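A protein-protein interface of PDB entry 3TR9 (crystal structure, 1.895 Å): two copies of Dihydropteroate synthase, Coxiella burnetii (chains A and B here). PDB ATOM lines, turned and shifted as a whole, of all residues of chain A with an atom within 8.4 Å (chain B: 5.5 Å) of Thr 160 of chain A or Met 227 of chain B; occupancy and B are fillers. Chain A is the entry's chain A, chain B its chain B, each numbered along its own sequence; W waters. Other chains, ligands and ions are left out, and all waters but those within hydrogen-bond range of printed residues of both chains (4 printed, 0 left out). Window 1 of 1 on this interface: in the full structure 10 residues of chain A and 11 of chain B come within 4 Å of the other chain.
Of the printed residues of chain B, Lys 162 of chain A touches Ala 226 (2.8 Å) and Met 227 (3.6 Å). Of the printed residues of chain A, Gln 180 of chain B touches Glu 159 (3.0 Å) and Thr 160 (3.6 Å). Gly 228 of chain B touches none of the printed residues of chain A. The nearest printed residue of chain B that does not touch Thr 160 of chain A is Ala 226 of chain B (4.5 Å). The nearest residue of chain A that does not touch Met 227 of chain B is Arg 161 of chain A (4.8 Å).
Among the printed residues, 9 pairs touch across the chains.
Water W4 lies within hydrogen-bond range of the side-chain hydroxyl of Ser 158 of chain A and the side-chain amino group of Lys 176 of chain B. Water W2 lies within hydrogen-bond range of OG1 of Thr 160 of chain A (2.5 Å), OG of Ser 158 of chain A (2.9 Å), NZ of Lys 176 of chain B (3.4 Å) and N of Glu 159 of chain A (3.4 Å). Water W1 lies within hydrogen-bond range of O of Glu 223 of chain B (2.8 Å), OG1 of Thr 160 of chain A (2.8 Å) and N of Arg 161 of chain A (3.5 Å). Water W3 bridges O of Thr 160 of chain A (2.9 Å) and NE2 of Gln 180 of chain B (3.1 Å).
Among the printed residues, merely in contact across the chains: Thr 160 of chain A with Met 227 of chain B (3.4 Å), Lys 162 of chain A with Met 227 of chain B (3.6 Å), Thr 160 of chain A with Lys 176 of chain B (3.6 Å), Thr 160 of chain A with Gln 180 of chain B (3.6 Å), Arg 161 of chain A with Ala 226 of chain B (3.7 Å) and Thr 160 of chain A with Lys 177 of chain B (3.999 Å).
No position is printed for both chains.
The backbone carbonyl oxygen (O) of Glu 159 of chain A is in hydrogen-bond range of the side-chain amide nitrogen (NE2) of Gln 180 of chain B. N of Lys 162 of chain A sits at hydrogen-bond distance from O of Ala 226 of chain B (2.8 Å). The side-chain hydroxyl of Ser 165 of chain A lies within hydrogen-bond range of the backbone carbonyl oxygen of Ala 226 of chain B (3.0 Å).
The backbone NH (N) of Arg 161 of chain A is in hydrogen-bond range of the side-chain hydroxyl (OG) of Ser 158 of chain A, at 3.2 Å. The guanidinium group (NH2) of Arg 161 of chain A is in hydrogen-bond range of the side-chain hydroxyl (OG1) of Thr 166 of chain A (3.4 Å). NH1 of Arg 161 of chain A lies within hydrogen-bond range of O of Gly 208 of chain A (3.0 Å). The side-chain hydroxyl of Ser 165 of chain A is in hydrogen-bond range of the backbone carbonyl oxygen of Lys 162 of chain A, at 2.8 Å. OE1 of Glu 223 of chain B is in salt-bridge range of NZ of Lys 176 of chain B (2.8 Å).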
ATOM      1  N   PHE A 156      26.979 -11.486 -25.471  1.00  0.00           N
ATOM      2  CA  PHE A 156      25.935 -10.873 -24.652  1.00  0.00           C
ATOM      3  C   PHE A 156      25.970 -11.415 -23.229  1.00  0.00           C
ATOM      4  O   PHE A 156      25.973 -12.630 -23.031  1.00  0.00           O
ATOM      5  CB  PHE A 156      24.555 -11.127 -25.262  1.00  0.00           C
ATOM      6  CG  PHE A 156      23.460 -10.310 -24.641  1.00  0.00           C
ATOM      7  CD1 PHE A 156      22.818 -10.746 -23.493  1.00  0.00           C
ATOM      8  CD2 PHE A 156      23.076  -9.100 -25.203  1.00  0.00           C
ATOM      9  CE1 PHE A 156      21.804  -9.992 -22.914  1.00  0.00           C
ATOM     10  CE2 PHE A 156      22.059  -8.345 -24.635  1.00  0.00           C
ATOM     11  CZ  PHE A 156      21.427  -8.790 -23.484  1.00  0.00           C
ATOM     12  N   PRO A 157      25.990 -10.514 -22.236  1.00  0.00           N
ATOM     13  CA  PRO A 157      26.062 -10.930 -20.828  1.00  0.00           C
ATOM     14  C   PRO A 157      24.737 -11.495 -20.353  1.00  0.00           C
ATOM     15  O   PRO A 157      23.763 -10.758 -20.178  1.00  0.00           O
ATOM     16  CB  PRO A 157      26.391  -9.625 -20.092  1.00  0.00           C
ATOM     17  CG  PRO A 157      25.878  -8.552 -20.959  1.00  0.00           C
ATOM     18  CD  PRO A 157      25.973  -9.047 -22.385  1.00  0.00           C
ATOM     19  N   SER A 158      24.699 -12.804 -20.162  1.00  0.00           N
ATOM     20  CA  SER A 158      23.484 -13.461 -19.719  1.00  0.00           C
ATOM     21  C   SER A 158      23.466 -13.604 -18.208  1.00  0.00           C
ATOM     22  O   SER A 158      24.159 -14.456 -17.650  1.00  0.00           O
ATOM     23  CB  SER A 158      23.359 -14.836 -20.365  1.00  0.00           C
ATOM     24  OG  SER A 158      22.352 -15.597 -19.723  1.00  0.00           O
ATOM     25  N   GLU A 159      22.664 -12.769 -17.555  1.00  0.00           N
ATOM     26  CA  GLU A 159      22.551 -12.771 -16.103  1.00  0.00           C
ATOM     27  C   GLU A 159      21.882 -14.025 -15.575  1.00  0.00           C
ATOM     28  O   GLU A 159      21.985 -14.320 -14.387  1.00  0.00           O
ATOM     29  CB  GLU A 159      21.727 -11.574 -15.635  1.00  0.00           C
ATOM     30  CG  GLU A 159      22.261 -10.236 -16.068  1.00  0.00           C
ATOM     31  CD  GLU A 159      21.283  -9.121 -15.772  1.00  0.00           C
ATOM     32  OE1 GLU A 159      20.154  -9.432 -15.333  1.00  0.00           O
ATOM     33  OE2 GLU A 159      21.640  -7.943 -15.975  1.00  0.00           O
ATOM     34  N   THR A 160      21.177 -14.748 -16.440  1.00  0.00           N
ATOM     35  CA  THR A 160      20.407 -15.902 -15.974  1.00  0.00           C
ATOM     36  C   THR A 160      21.072 -17.256 -16.234  1.00  0.00           C
ATOM     37  O   THR A 160      20.633 -18.268 -15.702  1.00  0.00           O
ATOM     38  CB  THR A 160      18.991 -15.927 -16.575  1.00  0.00           C
ATOM     39  OG1 THR A 160      19.077 -16.122 -17.992  1.00  0.00           O
ATOM     40  CG2 THR A 160      18.249 -14.616 -16.276  1.00  0.00           C
ATOM     41  N   ARG A 161      22.115 -17.290 -17.054  1.00  0.00           N
ATOM     42  CA  ARG A 161      22.754 -18.567 -17.340  1.00  0.00           C
ATOM     43  C   ARG A 161      23.398 -19.114 -16.079  1.00  0.00           C
ATOM     44  O   ARG A 161      24.021 -18.373 -15.329  1.00  0.00           O
ATOM     45  CB  ARG A 161      23.818 -18.438 -18.435  1.00  0.00           C
ATOM     46  CG  ARG A 161      24.668 -19.690 -18.562  1.00  0.00           C
ATOM     47  CD  ARG A 161      25.578 -19.702 -19.777  1.00  0.00           C
ATOM     48  NE  ARG A 161      26.186 -21.026 -19.931  1.00  0.00           N
ATOM     49  CZ  ARG A 161      27.337 -21.406 -19.376  1.00  0.00           C
ATOM     50  NH1 ARG A 161      28.044 -20.563 -18.630  1.00  0.00           N
ATOM     51  NH2 ARG A 161      27.784 -22.640 -19.572  1.00  0.00           N
ATOM     52  N   LYS A 162      23.238 -20.408 -15.838  1.00  0.00           N
ATOM     53  CA  LYS A 162      23.964 -21.038 -14.740  1.00  0.00           C
ATOM     54  C   LYS A 162      25.290 -21.581 -15.258  1.00  0.00           C
ATOM     55  O   LYS A 162      25.316 -22.500 -16.079  1.00  0.00           O
ATOM     56  CB  LYS A 162      23.151 -22.146 -14.081  1.00  0.00           C
ATOM     57  CG  LYS A 162      23.936 -22.859 -12.982  1.00  0.00           C
ATOM     58  CD  LYS A 162      23.061 -23.748 -12.126  1.00  0.00           C
ATOM     59  CE  LYS A 162      23.906 -24.433 -11.055  1.00  0.00           C
ATOM     60  NZ  LYS A 162      23.079 -25.066  -9.996  1.00  0.00           N
ATOM     61  N   PRO A 163      26.404 -20.991 -14.808  1.00  0.00           N
ATOM     62  CA  PRO A 163      27.700 -21.480 -15.291  1.00  0.00           C
ATOM     63  C   PRO A 163      27.850 -22.974 -15.029  1.00  0.00           C
ATOM     64  O   PRO A 163      27.417 -23.458 -13.983  1.00  0.00           O
ATOM     65  CB  PRO A 163      28.705 -20.684 -14.451  1.00  0.00           C
ATOM     66  CG  PRO A 163      27.990 -19.409 -14.141  1.00  0.00           C
ATOM     67  CD  PRO A 163      26.552 -19.837 -13.901  1.00  0.00           C
ATOM     68  N   SER A 165      26.399 -25.289 -16.777  1.00  0.00           N
ATOM     69  CA  SER A 165      25.183 -25.998 -17.197  1.00  0.00           C
ATOM     70  C   SER A 165      25.354 -26.702 -18.544  1.00  0.00           C
ATOM     71  O   SER A 165      24.527 -27.523 -18.936  1.00  0.00           O
ATOM     72  CB  SER A 165      23.969 -25.058 -17.227  1.00  0.00           C
ATOM     73  OG  SER A 165      24.153 -24.023 -18.178  1.00  0.00           O
ATOM     74  N   THR A 166      26.422 -26.359 -19.255  1.00  0.00           N
ATOM     75  CA  THR A 166      26.887 -27.152 -20.387  1.00  0.00           C
ATOM     76  C   THR A 166      28.384 -27.358 -20.218  1.00  0.00           C
ATOM     77  O   THR A 166      29.008 -26.707 -19.379  1.00  0.00           O
ATOM     78  CB  THR A 166      26.588 -26.485 -21.748  1.00  0.00           C
ATOM     79  OG1 THR A 166      26.974 -25.105 -21.713  1.00  0.00           O
ATOM     80  CG2 THR A 166      25.105 -26.573 -22.073  1.00  0.00           C
ATOM     81  N   GLY A 205      29.776 -12.925 -12.738  1.00  0.00           N
ATOM     82  CA  GLY A 205      28.591 -12.139 -12.431  1.00  0.00           C
ATOM     83  C   GLY A 205      27.598 -12.146 -13.587  1.00  0.00           C
ATOM     84  O   GLY A 205      27.207 -13.215 -14.068  1.00  0.00           O
ATOM     85  N   ASN A 206      27.199 -10.958 -14.044  1.00  0.00           N
ATOM     86  CA  ASN A 206      26.218 -10.840 -15.122  1.00  0.00           C
ATOM     87  C   ASN A 206      26.736 -11.357 -16.449  1.00  0.00           C
ATOM     88  O   ASN A 206      25.971 -11.478 -17.403  1.00  0.00           O
ATOM     89  CB  ASN A 206      25.783  -9.384 -15.317  1.00  0.00           C
ATOM     90  CG  ASN A 206      25.053  -8.831 -14.119  1.00  0.00           C
ATOM     91  OD1 ASN A 206      24.358  -9.560 -13.409  1.00  0.00           O
ATOM     92  ND2 ASN A 206      25.201  -7.531 -13.888  1.00  0.00           N
ATOM     93  N   TYR A 207      28.039 -11.631 -16.526  1.00  0.00           N
ATOM     94  CA  TYR A 207      28.609 -12.139 -17.766  1.00  0.00           C
ATOM     95  C   TYR A 207      28.363 -13.643 -17.932  1.00  0.00           C
ATOM     96  O   TYR A 207      28.778 -14.230 -18.925  1.00  0.00           O
ATOM     97  CB  TYR A 207      30.110 -11.828 -17.857  1.00  0.00           C
ATOM     98  CG  TYR A 207      30.421 -10.431 -18.368  1.00  0.00           C
ATOM     99  CD1 TYR A 207      29.512  -9.391 -18.218  1.00  0.00           C
ATOM    100  CD2 TYR A 207      31.617 -10.165 -19.023  1.00  0.00           C
ATOM    101  CE1 TYR A 207      29.799  -8.115 -18.688  1.00  0.00           C
ATOM    102  CE2 TYR A 207      31.910  -8.894 -19.505  1.00  0.00           C
ATOM    103  CZ  TYR A 207      30.999  -7.876 -19.333  1.00  0.00           C
ATOM    104  OH  TYR A 207      31.301  -6.620 -19.808  1.00  0.00           O
ATOM    105  N   GLY A 208      27.706 -14.259 -16.953  1.00  0.00           N
ATOM    106  CA  GLY A 208      27.249 -15.637 -17.088  1.00  0.00           C
ATOM    107  C   GLY A 208      28.308 -16.691 -17.379  1.00  0.00           C
ATOM    108  O   GLY A 208      28.068 -17.631 -18.150  1.00  0.00           O
ATOM    109  N   LYS B 176      13.213 -14.372 -19.034  1.00  0.00           N
ATOM    110  CA  LYS B 176      14.273 -15.065 -18.293  1.00  0.00           C
ATOM    111  C   LYS B 176      14.559 -14.388 -16.949  1.00  0.00           C
ATOM    112  O   LYS B 176      14.702 -15.050 -15.925  1.00  0.00           O
ATOM    113  CB  LYS B 176      15.551 -15.178 -19.137  1.00  0.00           C
ATOM    114  CG  LYS B 176      15.347 -15.983 -20.421  1.00  0.00           C
ATOM    115  CD  LYS B 176      16.667 -16.334 -21.099  1.00  0.00           C
ATOM    116  CE  LYS B 176      17.496 -15.104 -21.407  1.00  0.00           C
ATOM    117  NZ  LYS B 176      18.829 -15.476 -21.975  1.00  0.00           N
ATOM    118  N   LYS B 177      14.624 -13.067 -16.946  1.00  0.00           N
ATOM    119  CA  LYS B 177      14.862 -12.330 -15.702  1.00  0.00           C
ATOM    120  C   LYS B 177      13.784 -12.616 -14.653  1.00  0.00           C
ATOM    121  O   LYS B 177      14.088 -12.824 -13.472  1.00  0.00           O
ATOM    122  CB  LYS B 177      14.929 -10.824 -15.986  1.00  0.00           C
ATOM    123  CG  LYS B 177      15.090  -9.955 -14.739  1.00  0.00           C
ATOM    124  CD  LYS B 177      14.982  -8.471 -15.094  1.00  0.00           C
ATOM    125  CE  LYS B 177      15.150  -7.580 -13.869  1.00  0.00           C
ATOM    126  NZ  LYS B 177      16.499  -7.730 -13.261  1.00  0.00           N
ATOM    127  N   LEU B 179      11.668 -15.261 -14.527  1.00  0.00           N
ATOM    128  CA  LEU B 179      11.826 -16.645 -14.094  1.00  0.00           C
ATOM    129  C   LEU B 179      12.967 -16.798 -13.090  1.00  0.00           C
ATOM    130  O   LEU B 179      12.830 -17.518 -12.100  1.00  0.00           O
ATOM    131  CB  LEU B 179      12.044 -17.577 -15.288  1.00  0.00           C
ATOM    132  CG  LEU B 179      10.766 -18.170 -15.872  1.00  0.00           C
ATOM    133  CD1 LEU B 179      11.084 -19.093 -17.035  1.00  0.00           C
ATOM    134  CD2 LEU B 179       9.992 -18.912 -14.789  1.00  0.00           C
ATOM    135  N   GLN B 180      14.089 -16.127 -13.336  1.00  0.00           N
ATOM    136  CA  GLN B 180      15.215 -16.190 -12.391  1.00  0.00           C
ATOM    137  C   GLN B 180      14.809 -15.660 -11.015  1.00  0.00           C
ATOM    138  O   GLN B 180      15.184 -16.222  -9.986  1.00  0.00           O
ATOM    139  CB  GLN B 180      16.419 -15.402 -12.909  1.00  0.00           C
ATOM    140  CG  GLN B 180      17.554 -15.303 -11.887  1.00  0.00           C
ATOM    141  CD  GLN B 180      18.772 -14.567 -12.416  1.00  0.00           C
ATOM    142  OE1 GLN B 180      18.698 -13.393 -12.776  1.00  0.00           O
ATOM    143  NE2 GLN B 180      19.903 -15.258 -12.463  1.00  0.00           N
ATOM    144  N   ILE B 183      12.782 -18.240  -9.270  1.00  0.00           N
ATOM    145  CA  ILE B 183      13.698 -19.264  -8.766  1.00  0.00           C
ATOM    146  C   ILE B 183      14.370 -18.792  -7.482  1.00  0.00           C
ATOM    147  O   ILE B 183      14.457 -19.540  -6.513  1.00  0.00           O
ATOM    148  CB  ILE B 183      14.768 -19.639  -9.814  1.00  0.00           C
ATOM    149  CG1 ILE B 183      14.119 -20.366 -11.002  1.00  0.00           C
ATOM    150  CG2 ILE B 183      15.866 -20.508  -9.182  1.00  0.00           C
ATOM    151  CD1 ILE B 183      15.019 -20.467 -12.225  1.00  0.00           C
ATOM    152  N   ILE B 198      11.021 -25.310 -14.290  1.00  0.00           N
ATOM    153  CA  ILE B 198      10.580 -24.047 -14.867  1.00  0.00           C
ATOM    154  C   ILE B 198       9.951 -24.238 -16.241  1.00  0.00           C
ATOM    155  O   ILE B 198      10.190 -25.239 -16.916  1.00  0.00           O
ATOM    156  CB  ILE B 198      11.705 -22.993 -14.938  1.00  0.00           C
ATOM    157  CG1 ILE B 198      12.777 -23.410 -15.944  1.00  0.00           C
ATOM    158  CG2 ILE B 198      12.299 -22.737 -13.544  1.00  0.00           C
ATOM    159  CD1 ILE B 198      13.781 -22.315 -16.223  1.00  0.00           C
ATOM    160  N   PRO B 222      16.860 -23.428 -25.540  1.00  0.00           N
ATOM    161  CA  PRO B 222      18.108 -23.792 -24.857  1.00  0.00           C
ATOM    162  C   PRO B 222      18.558 -22.717 -23.873  1.00  0.00           C
ATOM    163  O   PRO B 222      19.319 -23.004 -22.957  1.00  0.00           O
ATOM    164  CB  PRO B 222      19.117 -23.923 -26.014  1.00  0.00           C
ATOM    165  CG  PRO B 222      18.275 -24.311 -27.186  1.00  0.00           C
ATOM    166  CD  PRO B 222      17.012 -23.477 -27.005  1.00  0.00           C
ATOM    167  N   GLU B 223      18.092 -21.489 -24.056  1.00  0.00           N
ATOM    168  CA  GLU B 223      18.427 -20.420 -23.120  1.00  0.00           C
ATOM    169  C   GLU B 223      17.744 -20.623 -21.772  1.00  0.00           C
ATOM    170  O   GLU B 223      18.268 -20.207 -20.735  1.00  0.00           O
ATOM    171  CB  GLU B 223      18.109 -19.046 -23.716  1.00  0.00           C
ATOM    172  CG  GLU B 223      18.909 -18.768 -24.982  1.00  0.00           C
ATOM    173  CD  GLU B 223      18.917 -17.306 -25.375  1.00  0.00           C
ATOM    174  OE1 GLU B 223      18.446 -16.469 -24.577  1.00  0.00           O
ATOM    175  OE2 GLU B 223      19.399 -16.994 -26.488  1.00  0.00           O
ATOM    176  N   PHE B 224      16.586 -21.278 -21.781  1.00  0.00           N
ATOM    177  CA  PHE B 224      15.930 -21.655 -20.524  1.00  0.00           C
ATOM    178  C   PHE B 224      16.609 -22.871 -19.897  1.00  0.00           C
ATOM    179  O   PHE B 224      16.819 -22.921 -18.683  1.00  0.00           O
ATOM    180  CB  PHE B 224      14.443 -21.933 -20.743  1.00  0.00           C
ATOM    181  CG  PHE B 224      13.657 -20.707 -21.134  1.00  0.00           C
ATOM    182  CD1 PHE B 224      13.164 -19.851 -20.163  1.00  0.00           C
ATOM    183  CD2 PHE B 224      13.432 -20.405 -22.465  1.00  0.00           C
ATOM    184  CE1 PHE B 224      12.457 -18.713 -20.511  1.00  0.00           C
ATOM    185  CE2 PHE B 224      12.711 -19.265 -22.825  1.00  0.00           C
ATOM    186  CZ  PHE B 224      12.229 -18.424 -21.844  1.00  0.00           C
ATOM    187  N   VAL B 225      16.958 -23.846 -20.731  1.00  0.00           N
ATOM    188  CA  VAL B 225      17.700 -25.012 -20.248  1.00  0.00           C
ATOM    189  C   VAL B 225      19.019 -24.574 -19.577  1.00  0.00           C
ATOM    190  O   VAL B 225      19.458 -25.178 -18.602  1.00  0.00           O
ATOM    191  CB  VAL B 225      17.962 -26.032 -21.389  1.00  0.00           C
ATOM    192  CG1 VAL B 225      18.789 -27.229 -20.879  1.00  0.00           C
ATOM    193  CG2 VAL B 225      16.641 -26.507 -22.000  1.00  0.00           C
ATOM    194  N   ALA B 226      19.617 -23.497 -20.080  1.00  0.00           N
ATOM    195  CA  ALA B 226      20.890 -22.989 -19.569  1.00  0.00           C
ATOM    196  C   ALA B 226      20.801 -22.453 -18.134  1.00  0.00           C
ATOM    197  O   ALA B 226      21.818 -22.194 -17.495  1.00  0.00           O
ATOM    198  CB  ALA B 226      21.442 -21.912 -20.499  1.00  0.00           C
ATOM    199  N   MET B 227      19.584 -22.290 -17.627  1.00  0.00           N
ATOM    200  CA  MET B 227      19.401 -21.812 -16.261  1.00  0.00           C
ATOM    201  C   MET B 227      19.604 -22.935 -15.246  1.00  0.00           C
ATOM    202  O   MET B 227      19.609 -22.695 -14.041  1.00  0.00           O
ATOM    203  CB  MET B 227      18.032 -21.119 -16.099  1.00  0.00           C
ATOM    204  CG  MET B 227      17.915 -19.867 -16.955  1.00  0.00           C
ATOM    205  SD  MET B 227      16.112 -19.074 -17.038  1.00  0.00           S
ATOM    206  CE  MET B 227      15.856 -18.735 -15.152  1.00  0.00           C
ATOM    207  N   GLY B 228      19.774 -24.160 -15.739  1.00  0.00           N
ATOM    208  CA  GLY B 228      20.251 -25.261 -14.917  1.00  0.00           C
ATOM    209  C   GLY B 228      19.212 -26.105 -14.198  1.00  0.00           C
ATOM    210  O   GLY B 228      19.550 -26.903 -13.324  1.00  0.00           O
ATOM    211  N   LEU B 229      17.945 -25.932 -14.561  1.00  0.00           N
ATOM    212  CA  LEU B 229      16.862 -26.699 -13.961  1.00  0.00           C
ATOM    213  C   LEU B 229      16.054 -27.404 -15.044  1.00  0.00           C
ATOM    214  O   LEU B 229      16.066 -26.993 -16.206  1.00  0.00           O
ATOM    215  CB  LEU B 229      15.932 -25.778 -13.162  1.00  0.00           C
ATOM    216  CG  LEU B 229      16.535 -25.042 -11.962  1.00  0.00           C
ATOM    217  CD1 LEU B 229      15.569 -23.985 -11.447  1.00  0.00           C
ATOM    218  CD2 LEU B 229      16.902 -26.029 -10.854  1.00  0.00           C
HETATM  219  O   HOH W   1      19.868 -18.335 -19.493  1.00  0.00           O
HETATM  220  O   HOH W   2      19.967 -14.074 -19.121  1.00  0.00           O
HETATM  221  O   HOH W   3      18.796 -17.957 -13.504  1.00  0.00           O
HETATM  222  O   HOH W   4      21.042 -17.026 -21.281  1.00  0.00           O
